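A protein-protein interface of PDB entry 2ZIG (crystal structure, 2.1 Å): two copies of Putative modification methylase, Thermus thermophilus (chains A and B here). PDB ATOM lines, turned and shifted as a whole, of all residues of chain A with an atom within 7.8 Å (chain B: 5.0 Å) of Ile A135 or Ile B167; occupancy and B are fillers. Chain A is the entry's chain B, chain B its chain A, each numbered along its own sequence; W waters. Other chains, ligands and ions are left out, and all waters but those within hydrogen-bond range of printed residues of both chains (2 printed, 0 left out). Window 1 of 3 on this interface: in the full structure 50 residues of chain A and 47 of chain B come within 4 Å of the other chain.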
ATOM      1  N   HIS A 116      -2.974  18.185 -23.709  1.00  0.00           N
ATOM      2  CA  HIS A 116      -2.367  19.420 -24.186  1.00  0.00           C
ATOM      3  C   HIS A 116      -2.741  19.707 -25.642  1.00  0.00           C
ATOM      4  O   HIS A 116      -2.942  20.862 -26.026  1.00  0.00           O
ATOM      5  CB  HIS A 116      -0.836  19.367 -24.052  1.00  0.00           C
ATOM      6  CG  HIS A 116      -0.148  18.735 -25.226  1.00  0.00           C
ATOM      7  ND1 HIS A 116      -0.071  17.369 -25.401  1.00  0.00           N
ATOM      8  CD2 HIS A 116       0.452  19.287 -26.307  1.00  0.00           C
ATOM      9  CE1 HIS A 116       0.548  17.107 -26.539  1.00  0.00           C
ATOM     10  NE2 HIS A 116       0.874  18.253 -27.108  1.00  0.00           N
ATOM     11  N   ASN A 132       4.497  28.839 -29.744  1.00  0.00           N
ATOM     12  CA  ASN A 132       5.189  27.609 -29.409  1.00  0.00           C
ATOM     13  C   ASN A 132       5.134  27.348 -27.911  1.00  0.00           C
ATOM     14  O   ASN A 132       5.329  28.246 -27.097  1.00  0.00           O
ATOM     15  CB  ASN A 132       6.647  27.659 -29.870  1.00  0.00           C
ATOM     16  CG  ASN A 132       6.830  27.067 -31.245  1.00  0.00           C
ATOM     17  OD1 ASN A 132       6.141  26.118 -31.610  1.00  0.00           O
ATOM     18  ND2 ASN A 132       7.766  27.610 -32.010  1.00  0.00           N
ATOM     19  N   PRO A 133       4.853  26.109 -27.525  1.00  0.00           N
ATOM     20  CA  PRO A 133       4.805  25.853 -26.087  1.00  0.00           C
ATOM     21  C   PRO A 133       6.222  25.704 -25.599  1.00  0.00           C
ATOM     22  O   PRO A 133       7.159  25.664 -26.398  1.00  0.00           O
ATOM     23  CB  PRO A 133       4.065  24.528 -26.006  1.00  0.00           C
ATOM     24  CG  PRO A 133       4.620  23.816 -27.200  1.00  0.00           C
ATOM     25  CD  PRO A 133       4.547  24.886 -28.284  1.00  0.00           C
ATOM     26  N   ILE A 134       6.364  25.634 -24.282  1.00  0.00           N
ATOM     27  CA  ILE A 134       7.653  25.402 -23.659  1.00  0.00           C
ATOM     28  C   ILE A 134       7.495  24.007 -23.038  1.00  0.00           C
ATOM     29  O   ILE A 134       6.444  23.683 -22.467  1.00  0.00           O
ATOM     30  CB  ILE A 134       7.964  26.442 -22.560  1.00  0.00           C
ATOM     31  CG1 ILE A 134       8.368  27.774 -23.206  1.00  0.00           C
ATOM     32  CG2 ILE A 134       9.091  25.929 -21.660  1.00  0.00           C
ATOM     33  CD1 ILE A 134       8.562  28.921 -22.212  1.00  0.00           C
ATOM     34  N   ILE A 135       8.525  23.179 -23.190  1.00  0.00           N
ATOM     35  CA  ILE A 135       8.505  21.832 -22.658  1.00  0.00           C
ATOM     36  C   ILE A 135       9.089  21.825 -21.261  1.00  0.00           C
ATOM     37  O   ILE A 135      10.247  22.166 -21.064  1.00  0.00           O
ATOM     38  CB  ILE A 135       9.338  20.852 -23.519  1.00  0.00           C
ATOM     39  CG1 ILE A 135       8.775  20.790 -24.938  1.00  0.00           C
ATOM     40  CG2 ILE A 135       9.327  19.449 -22.872  1.00  0.00           C
ATOM     41  CD1 ILE A 135       7.268  20.590 -24.985  1.00  0.00           C
ATOM     42  N   TRP A 136       8.282  21.442 -20.286  1.00  0.00           N
ATOM     43  CA  TRP A 136       8.778  21.375 -18.930  1.00  0.00           C
ATOM     44  C   TRP A 136       9.283  19.968 -18.661  1.00  0.00           C
ATOM     45  O   TRP A 136       8.488  19.053 -18.443  1.00  0.00           O
ATOM     46  CB  TRP A 136       7.672  21.723 -17.938  1.00  0.00           C
ATOM     47  CG  TRP A 136       8.090  21.556 -16.505  1.00  0.00           C
ATOM     48  CD1 TRP A 136       9.358  21.681 -15.989  1.00  0.00           C
ATOM     49  CD2 TRP A 136       7.230  21.291 -15.393  1.00  0.00           C
ATOM     50  NE1 TRP A 136       9.330  21.513 -14.625  1.00  0.00           N
ATOM     51  CE2 TRP A 136       8.038  21.271 -14.234  1.00  0.00           C
ATOM     52  CE3 TRP A 136       5.851  21.072 -15.263  1.00  0.00           C
ATOM     53  CZ2 TRP A 136       7.511  21.036 -12.962  1.00  0.00           C
ATOM     54  CZ3 TRP A 136       5.328  20.839 -13.996  1.00  0.00           C
ATOM     55  CH2 TRP A 136       6.159  20.823 -12.864  1.00  0.00           C
ATOM     56  N   HIS A 137      10.603  19.791 -18.686  1.00  0.00           N
ATOM     57  CA  HIS A 137      11.177  18.482 -18.416  1.00  0.00           C
ATOM     58  C   HIS A 137      11.139  18.347 -16.904  1.00  0.00           C
ATOM     59  O   HIS A 137      12.066  18.728 -16.192  1.00  0.00           O
ATOM     60  CB  HIS A 137      12.609  18.384 -18.941  1.00  0.00           C
ATOM     61  CG  HIS A 137      13.088  16.975 -19.090  1.00  0.00           C
ATOM     62  ND1 HIS A 137      14.331  16.659 -19.593  1.00  0.00           N
ATOM     63  CD2 HIS A 137      12.482  15.797 -18.818  1.00  0.00           C
ATOM     64  CE1 HIS A 137      14.468  15.345 -19.626  1.00  0.00           C
ATOM     65  NE2 HIS A 137      13.360  14.799 -19.162  1.00  0.00           N
ATOM     66  N   LYS A 138      10.012  17.825 -16.451  1.00  0.00           N
ATOM     67  CA  LYS A 138       9.681  17.626 -15.051  1.00  0.00           C
ATOM     68  C   LYS A 138      10.582  16.598 -14.385  1.00  0.00           C
ATOM     69  O   LYS A 138      11.260  16.897 -13.404  1.00  0.00           O
ATOM     70  CB  LYS A 138       8.221  17.166 -14.973  1.00  0.00           C
ATOM     71  CG  LYS A 138       7.453  17.508 -13.712  1.00  0.00           C
ATOM     72  CD  LYS A 138       6.009  17.006 -13.849  1.00  0.00           C
ATOM     73  CE  LYS A 138       5.154  17.319 -12.624  1.00  0.00           C
ATOM     74  NZ  LYS A 138       5.616  16.639 -11.378  1.00  0.00           N
ATOM     75  N   GLU A 166       8.013  12.108 -18.762  1.00  0.00           N
ATOM     76  CA  GLU A 166       8.997  12.973 -18.126  1.00  0.00           C
ATOM     77  C   GLU A 166       8.644  14.442 -18.315  1.00  0.00           C
ATOM     78  O   GLU A 166       9.314  15.306 -17.764  1.00  0.00           O
ATOM     79  CB  GLU A 166      10.373  12.749 -18.740  1.00  0.00           C
ATOM     80  CG  GLU A 166      10.911  11.354 -18.599  1.00  0.00           C
ATOM     81  CD  GLU A 166      12.117  11.130 -19.473  1.00  0.00           C
ATOM     82  OE1 GLU A 166      12.918  12.073 -19.632  1.00  0.00           O
ATOM     83  OE2 GLU A 166      12.275  10.008 -19.997  1.00  0.00           O
ATOM     84  N   ILE A 167       7.597  14.730 -19.077  1.00  0.00           N
ATOM     85  CA  ILE A 167       7.269  16.122 -19.363  1.00  0.00           C
ATOM     86  C   ILE A 167       5.822  16.577 -19.209  1.00  0.00           C
ATOM     87  O   ILE A 167       4.894  15.780 -19.077  1.00  0.00           O
ATOM     88  CB  ILE A 167       7.659  16.473 -20.825  1.00  0.00           C
ATOM     89  CG1 ILE A 167       6.735  15.705 -21.789  1.00  0.00           C
ATOM     90  CG2 ILE A 167       9.130  16.099 -21.094  1.00  0.00           C
ATOM     91  CD1 ILE A 167       6.837  16.104 -23.256  1.00  0.00           C
ATOM     92  N   GLU A 168       5.669  17.897 -19.249  1.00  0.00           N
ATOM     93  CA  GLU A 168       4.380  18.562 -19.231  1.00  0.00           C
ATOM     94  C   GLU A 168       4.534  19.673 -20.259  1.00  0.00           C
ATOM     95  O   GLU A 168       5.652  20.071 -20.587  1.00  0.00           O
ATOM     96  CB  GLU A 168       4.042  19.120 -17.855  1.00  0.00           C
ATOM     97  CG  GLU A 168       3.492  18.053 -16.938  1.00  0.00           C
ATOM     98  CD  GLU A 168       2.875  18.626 -15.696  1.00  0.00           C
ATOM     99  OE1 GLU A 168       2.236  19.696 -15.798  1.00  0.00           O
ATOM    100  OE2 GLU A 168       3.016  17.998 -14.626  1.00  0.00           O
ATOM    101  N   TYR A 169       3.417  20.162 -20.777  1.00  0.00           N
ATOM    102  CA  TYR A 169       3.449  21.178 -21.811  1.00  0.00           C
ATOM    103  C   TYR A 169       3.008  22.544 -21.308  1.00  0.00           C
ATOM    104  O   TYR A 169       2.002  22.664 -20.621  1.00  0.00           O
ATOM    105  CB  TYR A 169       2.538  20.751 -22.966  1.00  0.00           C
ATOM    106  CG  TYR A 169       2.814  19.358 -23.493  1.00  0.00           C
ATOM    107  CD1 TYR A 169       3.658  19.153 -24.582  1.00  0.00           C
ATOM    108  CD2 TYR A 169       2.256  18.243 -22.876  1.00  0.00           C
ATOM    109  CE1 TYR A 169       3.941  17.854 -25.047  1.00  0.00           C
ATOM    110  CE2 TYR A 169       2.530  16.953 -23.327  1.00  0.00           C
ATOM    111  CZ  TYR A 169       3.373  16.766 -24.411  1.00  0.00           C
ATOM    112  OH  TYR A 169       3.639  15.486 -24.847  1.00  0.00           O
ATOM    113  N   ILE A 170       3.770  23.576 -21.641  1.00  0.00           N
ATOM    114  CA  ILE A 170       3.378  24.911 -21.225  1.00  0.00           C
ATOM    115  C   ILE A 170       2.873  25.578 -22.481  1.00  0.00           C
ATOM    116  O   ILE A 170       3.649  26.095 -23.271  1.00  0.00           O
ATOM    117  CB  ILE A 170       4.551  25.705 -20.622  1.00  0.00           C
ATOM    118  CG1 ILE A 170       5.066  24.978 -19.376  1.00  0.00           C
ATOM    119  CG2 ILE A 170       4.082  27.112 -20.223  1.00  0.00           C
ATOM    120  CD1 ILE A 170       6.280  25.640 -18.730  1.00  0.00           C
ATOM    121  N   LEU A 171       1.556  25.515 -22.665  1.00  0.00           N
ATOM    122  CA  LEU A 171       0.886  26.089 -23.826  1.00  0.00           C
ATOM    123  C   LEU A 171       0.842  27.605 -23.762  1.00  0.00           C
ATOM    124  O   LEU A 171       0.626  28.185 -22.707  1.00  0.00           O
ATOM    125  CB  LEU A 171      -0.530  25.527 -23.924  1.00  0.00           C
ATOM    126  CG  LEU A 171      -0.588  23.994 -23.918  1.00  0.00           C
ATOM    127  CD1 LEU A 171      -2.037  23.521 -23.913  1.00  0.00           C
ATOM    128  CD2 LEU A 171       0.141  23.465 -25.135  1.00  0.00           C
ATOM    129  N   MET A 172       1.048  28.241 -24.907  1.00  0.00           N
ATOM    130  CA  MET A 172       1.039  29.693 -24.998  1.00  0.00           C
ATOM    131  C   MET A 172      -0.029  30.106 -26.007  1.00  0.00           C
ATOM    132  O   MET A 172       0.099  29.848 -27.207  1.00  0.00           O
ATOM    133  CB  MET A 172       2.411  30.187 -25.456  1.00  0.00           C
ATOM    134  CG  MET A 172       3.573  29.665 -24.625  1.00  0.00           C
ATOM    135  SD  MET A 172       3.885  30.656 -23.167  1.00  0.00           S
ATOM    136  CE  MET A 172       5.451  29.970 -22.609  1.00  0.00           C
ATOM    137  N   ARG A 202      13.703  29.862 -23.742  1.00  0.00           N
ATOM    138  CA  ARG A 202      14.190  28.718 -24.497  1.00  0.00           C
ATOM    139  C   ARG A 202      13.002  27.769 -24.518  1.00  0.00           C
ATOM    140  O   ARG A 202      12.086  27.921 -23.712  1.00  0.00           O
ATOM    141  CB  ARG A 202      15.399  28.082 -23.817  1.00  0.00           C
ATOM    142  CG  ARG A 202      15.168  27.660 -22.387  1.00  0.00           C
ATOM    143  CD  ARG A 202      16.390  26.916 -21.881  1.00  0.00           C
ATOM    144  NE  ARG A 202      17.571  27.766 -21.833  1.00  0.00           N
ATOM    145  CZ  ARG A 202      18.778  27.394 -22.250  1.00  0.00           C
ATOM    146  NH1 ARG A 202      19.803  28.238 -22.160  1.00  0.00           N
ATOM    147  NH2 ARG A 202      18.960  26.193 -22.780  1.00  0.00           N
ATOM    148  N   GLN A 203      12.997  26.800 -25.422  1.00  0.00           N
ATOM    149  CA  GLN A 203      11.846  25.924 -25.521  1.00  0.00           C
ATOM    150  C   GLN A 203      11.780  24.762 -24.534  1.00  0.00           C
ATOM    151  O   GLN A 203      10.733  24.143 -24.384  1.00  0.00           O
ATOM    152  CB  GLN A 203      11.691  25.421 -26.968  1.00  0.00           C
ATOM    153  CG  GLN A 203      10.445  24.571 -27.175  1.00  0.00           C
ATOM    154  CD  GLN A 203       9.911  24.599 -28.601  1.00  0.00           C
ATOM    155  OE1 GLN A 203      10.666  24.524 -29.569  1.00  0.00           O
ATOM    156  NE2 GLN A 203       8.601  24.684 -28.728  1.00  0.00           N
ATOM    157  N   ILE A 204      12.879  24.466 -23.850  1.00  0.00           N
ATOM    158  CA  ILE A 204      12.862  23.374 -22.880  1.00  0.00           C
ATOM    159  C   ILE A 204      13.433  23.813 -21.531  1.00  0.00           C
ATOM    160  O   ILE A 204      14.526  24.385 -21.460  1.00  0.00           O
ATOM    161  CB  ILE A 204      13.659  22.148 -23.407  1.00  0.00           C
ATOM    162  CG1 ILE A 204      13.030  21.655 -24.711  1.00  0.00           C
ATOM    163  CG2 ILE A 204      13.648  21.007 -22.378  1.00  0.00           C
ATOM    164  CD1 ILE A 204      13.729  20.446 -25.323  1.00  0.00           C
ATOM    165  N   TRP A 205      12.664  23.583 -20.469  1.00  0.00           N
ATOM    166  CA  TRP A 205      13.095  23.917 -19.115  1.00  0.00           C
ATOM    167  C   TRP A 205      13.391  22.602 -18.401  1.00  0.00           C
ATOM    168  O   TRP A 205      12.480  21.815 -18.136  1.00  0.00           O
ATOM    169  CB  TRP A 205      11.994  24.672 -18.355  1.00  0.00           C
ATOM    170  CG  TRP A 205      11.770  26.086 -18.832  1.00  0.00           C
ATOM    171  CD1 TRP A 205      12.507  26.764 -19.763  1.00  0.00           C
ATOM    172  CD2 TRP A 205      10.766  27.002 -18.372  1.00  0.00           C
ATOM    173  NE1 TRP A 205      12.028  28.038 -19.909  1.00  0.00           N
ATOM    174  CE2 TRP A 205      10.960  28.213 -19.069  1.00  0.00           C
ATOM    175  CE3 TRP A 205       9.720  26.915 -17.441  1.00  0.00           C
ATOM    176  CZ2 TRP A 205      10.141  29.343 -18.863  1.00  0.00           C
ATOM    177  CZ3 TRP A 205       8.907  28.029 -17.238  1.00  0.00           C
ATOM    178  CH2 TRP A 205       9.123  29.229 -17.948  1.00  0.00           C
ATOM    179  N   ASP A 206      14.661  22.359 -18.090  1.00  0.00           N
ATOM    180  CA  ASP A 206      15.034  21.117 -17.421  1.00  0.00           C
ATOM    181  C   ASP A 206      15.667  21.356 -16.061  1.00  0.00           C
ATOM    182  O   ASP A 206      16.205  20.430 -15.447  1.00  0.00           O
ATOM    183  CB  ASP A 206      15.998  20.316 -18.304  1.00  0.00           C
ATOM    184  CG  ASP A 206      17.339  21.005 -18.488  1.00  0.00           C
ATOM    185  OD1 ASP A 206      17.470  22.187 -18.108  1.00  0.00           O
ATOM    186  OD2 ASP A 206      18.266  20.364 -19.026  1.00  0.00           O
ATOM    187  N   ASP A 207      15.584  22.594 -15.587  1.00  0.00           N
ATOM    188  CA  ASP A 207      16.172  22.958 -14.302  1.00  0.00           C
ATOM    189  C   ASP A 207      15.147  23.168 -13.188  1.00  0.00           C
ATOM    190  O   ASP A 207      15.462  23.764 -12.161  1.00  0.00           O
ATOM    191  CB  ASP A 207      17.017  24.222 -14.464  1.00  0.00           C
ATOM    192  CG  ASP A 207      16.213  25.400 -14.999  1.00  0.00           C
ATOM    193  OD1 ASP A 207      15.113  25.182 -15.556  1.00  0.00           O
ATOM    194  OD2 ASP A 207      16.690  26.551 -14.876  1.00  0.00           O
ATOM    195  N   GLY B  98       7.151  18.857 -36.934  1.00  0.00           N
ATOM    196  CA  GLY B  98       7.622  20.101 -36.363  1.00  0.00           C
ATOM    197  C   GLY B  98       6.479  21.066 -36.633  1.00  0.00           C
ATOM    198  O   GLY B  98       5.870  21.007 -37.696  1.00  0.00           O
ATOM    199  N   ILE B 135      10.142  13.834 -27.672  1.00  0.00           N
ATOM    200  CA  ILE B 135      10.495  15.174 -28.110  1.00  0.00           C
ATOM    201  C   ILE B 135      11.864  15.152 -28.766  1.00  0.00           C
ATOM    202  O   ILE B 135      12.851  14.716 -28.158  1.00  0.00           O
ATOM    203  CB  ILE B 135      10.562  16.169 -26.928  1.00  0.00           C
ATOM    204  CG1 ILE B 135       9.219  16.218 -26.184  1.00  0.00           C
ATOM    205  CG2 ILE B 135      10.971  17.542 -27.444  1.00  0.00           C
ATOM    206  CD1 ILE B 135       8.013  16.544 -27.060  1.00  0.00           C
ATOM    207  N   TRP B 136      11.935  15.608 -30.009  1.00  0.00           N
ATOM    208  CA  TRP B 136      13.220  15.650 -30.687  1.00  0.00           C
ATOM    209  C   TRP B 136      13.784  17.054 -30.528  1.00  0.00           C
ATOM    210  O   TRP B 136      13.334  17.989 -31.189  1.00  0.00           O
ATOM    211  CB  TRP B 136      13.079  15.311 -32.175  1.00  0.00           C
ATOM    212  CG  TRP B 136      14.381  15.394 -32.934  1.00  0.00           C
ATOM    213  CD1 TRP B 136      15.647  15.286 -32.415  1.00  0.00           C
ATOM    214  CD2 TRP B 136      14.545  15.592 -34.344  1.00  0.00           C
ATOM    215  NE1 TRP B 136      16.580  15.408 -33.416  1.00  0.00           N
ATOM    216  CE2 TRP B 136      15.935  15.599 -34.608  1.00  0.00           C
ATOM    217  CE3 TRP B 136      13.650  15.766 -35.414  1.00  0.00           C
ATOM    218  CZ2 TRP B 136      16.456  15.776 -35.899  1.00  0.00           C
ATOM    219  CZ3 TRP B 136      14.170  15.940 -36.704  1.00  0.00           C
ATOM    220  CH2 TRP B 136      15.558  15.944 -36.931  1.00  0.00           C
ATOM    221  N   HIS B 137      14.751  17.202 -29.626  1.00  0.00           N
ATOM    222  CA  HIS B 137      15.380  18.490 -29.400  1.00  0.00           C
ATOM    223  C   HIS B 137      16.434  18.650 -30.486  1.00  0.00           C
ATOM    224  O   HIS B 137      17.583  18.268 -30.296  1.00  0.00           O
ATOM    225  CB  HIS B 137      16.029  18.528 -28.018  1.00  0.00           C
ATOM    226  CG  HIS B 137      16.394  19.906 -27.554  1.00  0.00           C
ATOM    227  ND1 HIS B 137      16.980  20.146 -26.329  1.00  0.00           N
ATOM    228  CD2 HIS B 137      16.229  21.119 -28.136  1.00  0.00           C
ATOM    229  CE1 HIS B 137      17.157  21.445 -26.173  1.00  0.00           C
ATOM    230  NE2 HIS B 137      16.709  22.060 -27.255  1.00  0.00           N
ATOM    231  N   LYS B 138      16.016  19.190 -31.629  1.00  0.00           N
ATOM    232  CA  LYS B 138      16.881  19.404 -32.790  1.00  0.00           C
ATOM    233  C   LYS B 138      17.960  20.448 -32.562  1.00  0.00           C
ATOM    234  O   LYS B 138      19.144  20.189 -32.784  1.00  0.00           O
ATOM    235  CB  LYS B 138      16.065  19.876 -33.990  1.00  0.00           C
ATOM    236  CG  LYS B 138      14.915  19.010 -34.386  1.00  0.00           C
ATOM    237  CD  LYS B 138      14.190  19.625 -35.576  1.00  0.00           C
ATOM    238  CE  LYS B 138      15.085  19.705 -36.796  1.00  0.00           C
ATOM    239  NZ  LYS B 138      14.343  20.245 -37.976  1.00  0.00           N
ATOM    240  N   THR B 165      11.850  28.072 -32.278  1.00  0.00           N
ATOM    241  CA  THR B 165      11.543  26.644 -32.283  1.00  0.00           C
ATOM    242  C   THR B 165      12.835  25.843 -32.151  1.00  0.00           C
ATOM    243  O   THR B 165      13.792  26.092 -32.876  1.00  0.00           O
ATOM    244  CB  THR B 165      10.865  26.221 -33.610  1.00  0.00           C
ATOM    245  OG1 THR B 165       9.745  27.072 -33.869  1.00  0.00           O
ATOM    246  CG2 THR B 165      10.390  24.769 -33.529  1.00  0.00           C
ATOM    247  N   GLU B 166      12.857  24.879 -31.235  1.00  0.00           N
ATOM    248  CA  GLU B 166      14.048  24.052 -31.025  1.00  0.00           C
ATOM    249  C   GLU B 166      13.727  22.568 -31.128  1.00  0.00           C
ATOM    250  O   GLU B 166      14.633  21.725 -31.162  1.00  0.00           O
ATOM    251  CB  GLU B 166      14.626  24.298 -29.633  1.00  0.00           C
ATOM    252  CG  GLU B 166      15.149  25.687 -29.358  1.00  0.00           C
ATOM    253  CD  GLU B 166      15.532  25.848 -27.897  1.00  0.00           C
ATOM    254  OE1 GLU B 166      16.191  24.928 -27.355  1.00  0.00           O
ATOM    255  OE2 GLU B 166      15.175  26.881 -27.290  1.00  0.00           O
ATOM    256  N   ILE B 167      12.440  22.252 -31.200  1.00  0.00           N
ATOM    257  CA  ILE B 167      12.008  20.865 -31.209  1.00  0.00           C
ATOM    258  C   ILE B 167      11.041  20.436 -32.295  1.00  0.00           C
ATOM    259  O   ILE B 167      10.403  21.250 -32.965  1.00  0.00           O
ATOM    260  CB  ILE B 167      11.277  20.532 -29.897  1.00  0.00           C
ATOM    261  CG1 ILE B 167       9.907  21.233 -29.914  1.00  0.00           C
ATOM    262  CG2 ILE B 167      12.108  20.987 -28.684  1.00  0.00           C
ATOM    263  CD1 ILE B 167       9.058  21.038 -28.682  1.00  0.00           C
ATOM    264  N   GLU B 168      10.941  19.119 -32.426  1.00  0.00           N
ATOM    265  CA  GLU B 168       9.996  18.481 -33.312  1.00  0.00           C
ATOM    266  C   GLU B 168       9.400  17.398 -32.430  1.00  0.00           C
ATOM    267  O   GLU B 168      10.024  16.978 -31.450  1.00  0.00           O
ATOM    268  CB  GLU B 168      10.665  17.898 -34.553  1.00  0.00           C
ATOM    269  CG  GLU B 168      10.823  18.947 -35.635  1.00  0.00           C
ATOM    270  CD  GLU B 168      11.178  18.368 -36.978  1.00  0.00           C
ATOM    271  OE1 GLU B 168      10.656  17.285 -37.316  1.00  0.00           O
ATOM    272  OE2 GLU B 168      11.964  19.006 -37.706  1.00  0.00           O
ATOM    273  N   TYR B 169       8.175  16.994 -32.753  1.00  0.00           N
ATOM    274  CA  TYR B 169       7.468  15.991 -31.986  1.00  0.00           C
ATOM    275  C   TYR B 169       7.445  14.664 -32.721  1.00  0.00           C
ATOM    276  O   TYR B 169       7.190  14.612 -33.933  1.00  0.00           O
ATOM    277  CB  TYR B 169       6.024  16.441 -31.729  1.00  0.00           C
ATOM    278  CG  TYR B 169       5.894  17.832 -31.147  1.00  0.00           C
ATOM    279  CD1 TYR B 169       6.112  18.968 -31.934  1.00  0.00           C
ATOM    280  CD2 TYR B 169       5.552  18.016 -29.810  1.00  0.00           C
ATOM    281  CE1 TYR B 169       5.988  20.254 -31.400  1.00  0.00           C
ATOM    282  CE2 TYR B 169       5.426  19.298 -29.265  1.00  0.00           C
ATOM    283  CZ  TYR B 169       5.640  20.407 -30.065  1.00  0.00           C
ATOM    284  OH  TYR B 169       5.477  21.666 -29.534  1.00  0.00           O
ATOM    285  N   ILE B 204      12.888  12.607 -24.217  1.00  0.00           N
ATOM    286  CA  ILE B 204      13.561  13.680 -24.945  1.00  0.00           C
ATOM    287  C   ILE B 204      14.886  13.211 -25.529  1.00  0.00           C
ATOM    288  O   ILE B 204      15.736  12.678 -24.808  1.00  0.00           O
ATOM    289  CB  ILE B 204      13.823  14.914 -24.027  1.00  0.00           C
ATOM    290  CG1 ILE B 204      12.493  15.528 -23.579  1.00  0.00           C
ATOM    291  CG2 ILE B 204      14.646  15.951 -24.754  1.00  0.00           C
ATOM    292  CD1 ILE B 204      12.649  16.759 -22.706  1.00  0.00           C
HETATM  293  O   HOH W   1      15.086  12.117 -21.653  1.00  0.00           O
HETATM  294  O   HOH W   2       6.616  23.351 -31.208  1.00  0.00           O
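OE1 of Gln A203 sits at hydrogen-bond distance from N of Ile B167.
The side-chain hydroxyl (OG1) of Thr B165 sits at hydrogen-bond distance from the side-chain amide nitrogen (ND2) of Asn A132 (2.8 Å).
OE1 of Gln A203 is in hydrogen-bond range of N of Glu B166 (2.8 Å).
Printed residues of chain A that touch a printed residue of chain B: Asn A132, Pro A133, Ile A135, His A137, Ile A167, Arg A202, Gln A203 and Ile A204.
Hydrophobic or aromatic side chains of chain A within 4 Å of the printed part of chain B: Pro A133, Ile A135, His A137, Ile A167 and Ile A204.
Hydrophobic or aromatic side chains of chain B that line the printed part of chain A: Ile B135, His B137, Ile B167, Tyr B169 and Ile B204.
Along chain B the printed residues that touch a printed residue of chain A span positions 135 to 204.
Among the printed residues, 12 pairs touch across the chains.
Tyr B169 touches Pro A133.
Ile A135 touches Ile B167.
CD1 of Ile B204 touches ND1 of His A137, 3.5 Å away.
Ile A167 touches Ile B135.
Ile A167 touches Ile B204.
Glu B166 touches Arg A202.
Gln A203 touches Thr B165.
ND1 of His B137 touches CD1 of Ile A204, 3.4 Å away.
Ile A204 touches Ile B167.
Of the printed residues of chain B, His A137 touches Ile B204.
Ile A170 touches none of the printed residues of chain B.
Printed residues of chain B within 4 Å of Arg A202: Glu B166 (3.5 Å).
Asp A206 touches none of the printed residues of chain B.
Ile B167 touches just these residues of chain A: Ile A135, Gln A203 and Ile A204.
The nearest residue of chain B that does not touch Ile A135 is Ile B204 (4.3 Å).
The nearest residue of chain A that does not touch Ile B167 is Pro A133 (5.4 Å).
The nearest printed residue of chain A that does not touch Ile B204 is Ile A135 (4.3 Å).
Ile A135 touches Ile B167, and with the chains exchanged Ile A167 touches Ile B135.
His A137 touches Ile B204, and with the chains exchanged Ile A204 touches His B137.
Ile A167 touches Ile B204, and with the chains exchanged Ile A204 touches Ile B167.
Positions printed for both chains: 135, 136, 137, 138, 166, 167, 168, 169 and 204.
Of the 12 pairs that touch across the chains among the printed residues, 6 have their exchanged pair printed and touching as well.
Water W2 lies within hydrogen-bond range of the side-chain hydroxyl (OH) of Tyr B169, the side-chain amide oxygen (OD1) of Asn A132 and the side-chain amide nitrogen (NE2) of Gln A203.
Water W1 lies within hydrogen-bond range of OE1 of Glu A166 (3.0 Å) and O of Ile B204 (3.3 Å).
The side-chain amide nitrogen (NE2) of Gln A203 is in hydrogen-bond range of the backbone carbonyl oxygen (O) of Pro A133 (2.9 Å).
The side-chain carboxylate (OE1) of Glu A166 sits at hydrogen-bond distance from a ring nitrogen (NE2) of His A137 (2.8 Å).
The backbone NH (N) of Ile A135 is in hydrogen-bond range of the backbone carbonyl oxygen (O) of Gln A203 (2.7 Å).
The backbone NH of Lys B138 sits at hydrogen-bond distance from the backbone carbonyl oxygen of Glu B166 (2.9 Å).
N of His A137 lies within hydrogen-bond range of O of Trp A205, 2.8 Å away.
NE2 of His B137 sits at hydrogen-bond distance from OE1 of Glu B166 (2.9 Å).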
